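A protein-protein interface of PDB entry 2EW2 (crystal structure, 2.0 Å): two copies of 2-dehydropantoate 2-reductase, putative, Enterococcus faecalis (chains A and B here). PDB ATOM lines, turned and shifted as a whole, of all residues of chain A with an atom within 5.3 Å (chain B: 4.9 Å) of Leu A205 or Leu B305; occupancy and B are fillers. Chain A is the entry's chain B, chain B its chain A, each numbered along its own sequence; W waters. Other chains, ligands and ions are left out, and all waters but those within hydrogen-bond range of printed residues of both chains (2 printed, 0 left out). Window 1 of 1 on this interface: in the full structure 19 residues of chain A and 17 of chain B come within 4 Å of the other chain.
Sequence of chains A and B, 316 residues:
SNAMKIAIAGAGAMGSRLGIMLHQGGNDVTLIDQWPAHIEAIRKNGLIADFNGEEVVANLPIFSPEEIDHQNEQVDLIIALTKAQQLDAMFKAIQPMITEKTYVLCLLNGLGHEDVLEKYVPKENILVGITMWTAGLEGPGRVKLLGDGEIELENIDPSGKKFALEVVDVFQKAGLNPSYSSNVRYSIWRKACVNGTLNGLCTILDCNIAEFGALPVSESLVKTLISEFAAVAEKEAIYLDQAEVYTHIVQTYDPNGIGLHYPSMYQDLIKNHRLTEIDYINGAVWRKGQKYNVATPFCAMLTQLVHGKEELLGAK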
ATOM      1  N   GLY A 200      27.373 -10.654 -14.877  1.00  0.00           N
ATOM      2  CA  GLY A 200      26.481 -11.083 -13.815  1.00  0.00           C
ATOM      3  C   GLY A 200      25.166 -11.574 -14.404  1.00  0.00           C
ATOM      4  O   GLY A 200      24.609 -12.552 -13.934  1.00  0.00           O
ATOM      5  N   LEU A 201      24.692 -10.903 -15.444  1.00  0.00           N
ATOM      6  CA  LEU A 201      23.395 -11.217 -16.054  1.00  0.00           C
ATOM      7  C   LEU A 201      23.348 -12.611 -16.701  1.00  0.00           C
ATOM      8  O   LEU A 201      22.414 -13.379 -16.452  1.00  0.00           O
ATOM      9  CB  LEU A 201      22.962 -10.115 -17.037  1.00  0.00           C
ATOM     10  CG  LEU A 201      22.596  -8.761 -16.398  1.00  0.00           C
ATOM     11  CD1 LEU A 201      22.512  -7.615 -17.436  1.00  0.00           C
ATOM     12  CD2 LEU A 201      21.308  -8.827 -15.590  1.00  0.00           C
ATOM     13  N   CYS A 202      24.355 -12.941 -17.507  1.00  0.00           N
ATOM     14  CA  CYS A 202      24.434 -14.263 -18.147  1.00  0.00           C
ATOM     15  C   CYS A 202      24.674 -15.343 -17.111  1.00  0.00           C
ATOM     16  O   CYS A 202      24.144 -16.453 -17.233  1.00  0.00           O
ATOM     17  CB  CYS A 202      25.526 -14.298 -19.223  1.00  0.00           C
ATOM     18  SG  CYS A 202      25.199 -13.204 -20.607  1.00  0.00           S
ATOM     19  N   THR A 203      25.462 -15.014 -16.085  1.00  0.00           N
ATOM     20  CA  THR A 203      25.695 -15.924 -14.952  1.00  0.00           C
ATOM     21  C   THR A 203      24.413 -16.267 -14.196  1.00  0.00           C
ATOM     22  O   THR A 203      24.153 -17.437 -13.897  1.00  0.00           O
ATOM     23  CB  THR A 203      26.763 -15.340 -13.974  1.00  0.00           C
ATOM     24  OG1 THR A 203      28.029 -15.298 -14.629  1.00  0.00           O
ATOM     25  CG2 THR A 203      26.911 -16.171 -12.707  1.00  0.00           C
ATOM     26  N   ILE A 204      23.619 -15.242 -13.880  1.00  0.00           N
ATOM     27  CA  ILE A 204      22.387 -15.425 -13.123  1.00  0.00           C
ATOM     28  C   ILE A 204      21.287 -16.087 -13.952  1.00  0.00           C
ATOM     29  O   ILE A 204      20.634 -17.028 -13.487  1.00  0.00           O
ATOM     30  CB  ILE A 204      21.907 -14.067 -12.501  1.00  0.00           C
ATOM     31  CG1 ILE A 204      22.786 -13.689 -11.294  1.00  0.00           C
ATOM     32  CG2 ILE A 204      20.466 -14.146 -12.069  1.00  0.00           C
ATOM     33  CD1 ILE A 204      22.898 -14.790 -10.187  1.00  0.00           C
ATOM     34  N   LEU A 205      21.094 -15.619 -15.179  1.00  0.00           N
ATOM     35  CA  LEU A 205      20.077 -16.192 -16.048  1.00  0.00           C
ATOM     36  C   LEU A 205      20.463 -17.545 -16.682  1.00  0.00           C
ATOM     37  O   LEU A 205      19.581 -18.276 -17.162  1.00  0.00           O
ATOM     38  CB  LEU A 205      19.680 -15.185 -17.133  1.00  0.00           C
ATOM     39  CG  LEU A 205      18.898 -13.937 -16.688  1.00  0.00           C
ATOM     40  CD1 LEU A 205      18.743 -12.940 -17.845  1.00  0.00           C
ATOM     41  CD2 LEU A 205      17.529 -14.372 -16.192  1.00  0.00           C
ATOM     42  N   ASP A 206      21.765 -17.864 -16.667  1.00  0.00           N
ATOM     43  CA  ASP A 206      22.345 -19.044 -17.354  1.00  0.00           C
ATOM     44  C   ASP A 206      22.082 -19.002 -18.853  1.00  0.00           C
ATOM     45  O   ASP A 206      21.198 -19.685 -19.343  1.00  0.00           O
ATOM     46  CB  ASP A 206      21.844 -20.379 -16.774  1.00  0.00           C
ATOM     47  CG  ASP A 206      22.698 -21.572 -17.221  1.00  0.00           C
ATOM     48  OD1 ASP A 206      23.392 -21.463 -18.243  1.00  0.00           O
ATOM     49  OD2 ASP A 206      22.695 -22.616 -16.541  1.00  0.00           O
ATOM     50  N   CYS A 207      22.834 -18.177 -19.571  1.00  0.00           N
ATOM     51  CA  CYS A 207      22.702 -18.065 -21.016  1.00  0.00           C
ATOM     52  C   CYS A 207      23.964 -17.435 -21.628  1.00  0.00           C
ATOM     53  O   CYS A 207      24.803 -16.884 -20.906  1.00  0.00           O
ATOM     54  CB  CYS A 207      21.457 -17.254 -21.375  1.00  0.00           C
ATOM     55  SG  CYS A 207      21.524 -15.489 -20.905  1.00  0.00           S
ATOM     56  N   PHE A 212      21.209 -13.706 -24.304  1.00  0.00           N
ATOM     57  CA  PHE A 212      20.855 -12.555 -23.473  1.00  0.00           C
ATOM     58  C   PHE A 212      20.414 -11.341 -24.303  1.00  0.00           C
ATOM     59  O   PHE A 212      19.354 -10.750 -24.052  1.00  0.00           O
ATOM     60  CB  PHE A 212      21.965 -12.139 -22.495  1.00  0.00           C
ATOM     61  CG  PHE A 212      21.576 -10.931 -21.696  1.00  0.00           C
ATOM     62  CD1 PHE A 212      20.744 -11.058 -20.587  1.00  0.00           C
ATOM     63  CD2 PHE A 212      21.932  -9.660 -22.122  1.00  0.00           C
ATOM     64  CE1 PHE A 212      20.312  -9.923 -19.887  1.00  0.00           C
ATOM     65  CE2 PHE A 212      21.495  -8.534 -21.425  1.00  0.00           C
ATOM     66  CZ  PHE A 212      20.697  -8.669 -20.324  1.00  0.00           C
ATOM     67  N   LEU A 215      16.770 -10.938 -25.599  1.00  0.00           N
ATOM     68  CA  LEU A 215      15.669 -10.861 -24.649  1.00  0.00           C
ATOM     69  C   LEU A 215      15.007  -9.497 -24.734  1.00  0.00           C
ATOM     70  O   LEU A 215      15.678  -8.508 -24.973  1.00  0.00           O
ATOM     71  CB  LEU A 215      16.154 -11.123 -23.213  1.00  0.00           C
ATOM     72  CG  LEU A 215      16.721 -12.506 -22.923  1.00  0.00           C
ATOM     73  CD1 LEU A 215      17.269 -12.584 -21.506  1.00  0.00           C
ATOM     74  CD2 LEU A 215      15.652 -13.589 -23.181  1.00  0.00           C
ATOM     75  N   VAL A 217      14.030  -7.748 -22.422  1.00  0.00           N
ATOM     76  CA  VAL A 217      14.436  -6.963 -21.251  1.00  0.00           C
ATOM     77  C   VAL A 217      15.930  -6.633 -21.269  1.00  0.00           C
ATOM     78  O   VAL A 217      16.440  -6.039 -20.317  1.00  0.00           O
ATOM     79  CB  VAL A 217      14.106  -7.704 -19.932  1.00  0.00           C
ATOM     80  CG1 VAL A 217      12.598  -7.927 -19.810  1.00  0.00           C
ATOM     81  CG2 VAL A 217      14.863  -9.032 -19.851  1.00  0.00           C
ATOM     82  N   LEU A 221      17.672  -3.782 -18.734  1.00  0.00           N
ATOM     83  CA  LEU A 221      18.656  -4.253 -17.771  1.00  0.00           C
ATOM     84  C   LEU A 221      20.013  -3.563 -17.998  1.00  0.00           C
ATOM     85  O   LEU A 221      20.604  -3.003 -17.061  1.00  0.00           O
ATOM     86  CB  LEU A 221      18.803  -5.775 -17.844  1.00  0.00           C
ATOM     87  CG  LEU A 221      17.653  -6.568 -17.226  1.00  0.00           C
ATOM     88  CD1 LEU A 221      17.739  -8.040 -17.661  1.00  0.00           C
ATOM     89  CD2 LEU A 221      17.613  -6.446 -15.687  1.00  0.00           C
ATOM     90  N   LEU A 305      22.771 -11.350  -5.727  1.00  0.00           N
ATOM     91  CA  LEU A 305      22.314 -12.559  -6.432  1.00  0.00           C
ATOM     92  C   LEU A 305      23.498 -13.447  -6.810  1.00  0.00           C
ATOM     93  O   LEU A 305      23.459 -14.664  -6.606  1.00  0.00           O
ATOM     94  CB  LEU A 305      21.509 -12.201  -7.696  1.00  0.00           C
ATOM     95  CG  LEU A 305      20.138 -11.517  -7.465  1.00  0.00           C
ATOM     96  CD1 LEU A 305      19.493 -11.157  -8.795  1.00  0.00           C
ATOM     97  CD2 LEU A 305      19.234 -12.414  -6.653  1.00  0.00           C
ATOM     98  N   ILE B 204      14.858 -17.564  -9.835  1.00  0.00           N
ATOM     99  CA  ILE B 204      16.045 -17.060 -10.497  1.00  0.00           C
ATOM    100  C   ILE B 204      17.310 -17.784 -10.039  1.00  0.00           C
ATOM    101  O   ILE B 204      18.151 -18.138 -10.864  1.00  0.00           O
ATOM    102  CB  ILE B 204      16.183 -15.507 -10.325  1.00  0.00           C
ATOM    103  CG1 ILE B 204      15.136 -14.768 -11.170  1.00  0.00           C
ATOM    104  CG2 ILE B 204      17.558 -15.052 -10.704  1.00  0.00           C
ATOM    105  CD1 ILE B 204      15.205 -15.033 -12.696  1.00  0.00           C
ATOM    106  N   MET B 301      13.965  -4.990 -11.213  1.00  0.00           N
ATOM    107  CA  MET B 301      14.973  -5.883 -11.755  1.00  0.00           C
ATOM    108  C   MET B 301      14.532  -7.350 -11.673  1.00  0.00           C
ATOM    109  O   MET B 301      14.754  -8.102 -12.598  1.00  0.00           O
ATOM    110  CB  MET B 301      16.323  -5.704 -11.049  1.00  0.00           C
ATOM    111  CG  MET B 301      17.351  -6.756 -11.501  1.00  0.00           C
ATOM    112  SD  MET B 301      19.134  -6.416 -10.725  1.00  0.00           S
ATOM    113  CE  MET B 301      19.537  -8.009 -10.235  1.00  0.00           C
ATOM    114  N   LEU B 302      13.941  -7.739 -10.553  1.00  0.00           N
ATOM    115  CA  LEU B 302      13.441  -9.098 -10.390  1.00  0.00           C
ATOM    116  C   LEU B 302      12.361  -9.435 -11.423  1.00  0.00           C
ATOM    117  O   LEU B 302      12.353 -10.534 -11.986  1.00  0.00           O
ATOM    118  CB  LEU B 302      12.934  -9.334  -8.957  1.00  0.00           C
ATOM    119  CG  LEU B 302      12.543 -10.777  -8.606  1.00  0.00           C
ATOM    120  CD1 LEU B 302      13.748 -11.751  -8.812  1.00  0.00           C
ATOM    121  CD2 LEU B 302      12.035 -10.840  -7.188  1.00  0.00           C
ATOM    122  N   THR B 303      11.475  -8.487 -11.687  1.00  0.00           N
ATOM    123  CA  THR B 303      10.456  -8.653 -12.722  1.00  0.00           C
ATOM    124  C   THR B 303      11.095  -8.886 -14.097  1.00  0.00           C
ATOM    125  O   THR B 303      10.710  -9.825 -14.829  1.00  0.00           O
ATOM    126  CB  THR B 303       9.517  -7.434 -12.758  1.00  0.00           C
ATOM    127  OG1 THR B 303       8.831  -7.352 -11.499  1.00  0.00           O
ATOM    128  CG2 THR B 303       8.517  -7.530 -13.898  1.00  0.00           C
ATOM    129  N   GLN B 304      12.070  -8.036 -14.436  1.00  0.00           N
ATOM    130  CA  GLN B 304      12.806  -8.139 -15.706  1.00  0.00           C
ATOM    131  C   GLN B 304      13.580  -9.463 -15.816  1.00  0.00           C
ATOM    132  O   GLN B 304      13.546 -10.115 -16.853  1.00  0.00           O
ATOM    133  CB  GLN B 304      13.759  -6.945 -15.866  1.00  0.00           C
ATOM    134  CG  GLN B 304      13.049  -5.617 -16.065  1.00  0.00           C
ATOM    135  CD  GLN B 304      14.004  -4.427 -16.065  1.00  0.00           C
ATOM    136  OE1 GLN B 304      14.947  -4.377 -16.853  1.00  0.00           O
ATOM    137  NE2 GLN B 304      13.753  -3.462 -15.198  1.00  0.00           N
ATOM    138  N   LEU B 305      14.266  -9.860 -14.744  1.00  0.00           N
ATOM    139  CA  LEU B 305      14.980 -11.140 -14.741  1.00  0.00           C
ATOM    140  C   LEU B 305      14.030 -12.350 -14.948  1.00  0.00           C
ATOM    141  O   LEU B 305      14.349 -13.269 -15.704  1.00  0.00           O
ATOM    142  CB  LEU B 305      15.770 -11.323 -13.449  1.00  0.00           C
ATOM    143  CG  LEU B 305      16.975 -10.389 -13.206  1.00  0.00           C
ATOM    144  CD1 LEU B 305      17.576 -10.756 -11.880  1.00  0.00           C
ATOM    145  CD2 LEU B 305      18.034 -10.509 -14.307  1.00  0.00           C
ATOM    146  N   VAL B 306      12.885 -12.343 -14.272  1.00  0.00           N
ATOM    147  CA  VAL B 306      11.887 -13.429 -14.438  1.00  0.00           C
ATOM    148  C   VAL B 306      11.328 -13.434 -15.871  1.00  0.00           C
ATOM    149  O   VAL B 306      11.250 -14.502 -16.487  1.00  0.00           O
ATOM    150  CB  VAL B 306      10.756 -13.376 -13.367  1.00  0.00           C
ATOM    151  CG1 VAL B 306       9.609 -14.387 -13.694  1.00  0.00           C
ATOM    152  CG2 VAL B 306      11.335 -13.686 -12.031  1.00  0.00           C
ATOM    153  N   HIS B 307      10.977 -12.259 -16.413  1.00  0.00           N
ATOM    154  CA  HIS B 307      10.593 -12.178 -17.825  1.00  0.00           C
ATOM    155  C   HIS B 307      11.706 -12.641 -18.782  1.00  0.00           C
ATOM    156  O   HIS B 307      11.415 -13.266 -19.786  1.00  0.00           O
ATOM    157  CB  HIS B 307      10.129 -10.783 -18.230  1.00  0.00           C
ATOM    158  CG  HIS B 307       8.783 -10.414 -17.687  1.00  0.00           C
ATOM    159  ND1 HIS B 307       7.787 -11.344 -17.448  1.00  0.00           N
ATOM    160  CD2 HIS B 307       8.261  -9.209 -17.364  1.00  0.00           C
ATOM    161  CE1 HIS B 307       6.718 -10.726 -16.979  1.00  0.00           C
ATOM    162  NE2 HIS B 307       6.980  -9.428 -16.919  1.00  0.00           N
ATOM    163  N   GLY B 308      12.959 -12.312 -18.476  1.00  0.00           N
ATOM    164  CA  GLY B 308      14.106 -12.819 -19.238  1.00  0.00           C
ATOM    165  C   GLY B 308      14.172 -14.347 -19.158  1.00  0.00           C
ATOM    166  O   GLY B 308      14.314 -15.023 -20.176  1.00  0.00           O
ATOM    167  N   LYS B 309      14.031 -14.887 -17.952  1.00  0.00           N
ATOM    168  CA  LYS B 309      14.056 -16.336 -17.734  1.00  0.00           C
ATOM    169  C   LYS B 309      12.911 -17.088 -18.463  1.00  0.00           C
ATOM    170  O   LYS B 309      13.134 -18.157 -19.046  1.00  0.00           O
ATOM    171  CB  LYS B 309      14.045 -16.641 -16.232  1.00  0.00           C
ATOM    172  CG  LYS B 309      14.411 -18.072 -15.854  1.00  0.00           C
ATOM    173  CD  LYS B 309      15.881 -18.364 -16.128  1.00  0.00           C
ATOM    174  CE  LYS B 309      16.248 -19.811 -15.798  1.00  0.00           C
ATOM    175  NZ  LYS B 309      17.684 -20.088 -16.143  1.00  0.00           N
ATOM    176  N   LEU B 312      13.878 -17.218 -22.053  1.00  0.00           N
ATOM    177  CA  LEU B 312      14.962 -18.183 -22.231  1.00  0.00           C
ATOM    178  C   LEU B 312      14.468 -19.629 -22.242  1.00  0.00           C
ATOM    179  O   LEU B 312      14.971 -20.442 -23.005  1.00  0.00           O
ATOM    180  CB  LEU B 312      16.049 -18.017 -21.170  1.00  0.00           C
ATOM    181  CG  LEU B 312      16.947 -16.778 -21.281  1.00  0.00           C
ATOM    182  CD1 LEU B 312      17.805 -16.594 -19.991  1.00  0.00           C
ATOM    183  CD2 LEU B 312      17.818 -16.803 -22.567  1.00  0.00           C
HETATM  184  O   HOH W   1      18.241 -20.331 -19.023  1.00  0.00           O
HETATM  185  O   HOH W   2      20.862 -18.547 -11.271  1.00  0.00           O
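The backbone NH (N) of Cys A207 lies within hydrogen-bond range of the backbone carbonyl oxygen (O) of Cys A202 (3.2 Å).
Leu A205 touches just these residues of chain B: Leu B305, Lys B309 and Leu B312. Leu B305 touches three residues of chain A. Of the printed residues of chain B, Leu A305 touches Met B301 and Leu B305. Of the printed residues of chain B, Val A217 touches Gln B304 and Gly B308. Printed residues of chain A within 4 Å of Gly B308: Leu A215 and Val A217. Printed residues of chain A within 4 Å of Met B301: Leu A305 (3.5 Å). Val B306 touches none of the printed residues of chain A. The nearest residue of chain B that does not touch Leu A205 is Ile B204 (4.2 Å). The nearest printed residue of chain B that does not touch Leu A305 is Ile B204 (4.7 Å).
OE1 of Gln B304 lies within hydrogen-bond range of N of Leu A221 (3.4 Å). The side-chain amino group of Lys B309 lies within hydrogen-bond range of the backbone carbonyl oxygen of Leu A205 (2.8 Å).
Ile A204 touches its own counterpart, Ile B204. Leu B305 touches its own counterpart, Leu A305. 2 positions are printed for both chains.
Water W2 bridges the backbone carbonyl oxygen of Ile A204 (2.7 Å) and the backbone carbonyl oxygen of Ile B204 (2.8 Å). Water W1 lies within hydrogen-bond range of the side-chain amino group (NZ) of Lys B309 (2.9 Å), the backbone carbonyl oxygen (O) of Asp A206 (3.0 Å) and the backbone carbonyl oxygen (O) of Leu A205 (3.1 Å).
Of the 13 printed residues of chain A, 8 touch a printed residue of chain B. Of the 11 printed residues of chain B, 7 touch a printed residue of chain A. Hydrophobic or aromatic side chains of chain B that line the printed part of chain A: Ile B204, Met B301, Leu B305 and Leu B312. Among the printed residues, no Asp or Glu carboxylate lies within 4 Å of a Lys or Arg side-chain nitrogen of the other chain.
Among the printed residues, pairs that only touch across the chains: Leu A201 with Leu B305 (3.9 Å), Ile A204 with Ile B204 (3.3 Å), Leu A205 with Leu B305 (3.4 Å), Leu A205 with Leu B312 (3.7 Å), Cys A207 with Leu B312 (3.9 Å), Leu A215 with Gly B308 (3.6 Å), Leu A215 with Leu B312 (3.9 Å), Val A217 with Gln B304 (3.4 Å), Val A217 with Gly B308 (3.9 Å), Leu A305 with Met B301 (3.5 Å) and Leu A305 with Leu B305 (3.7 Å).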
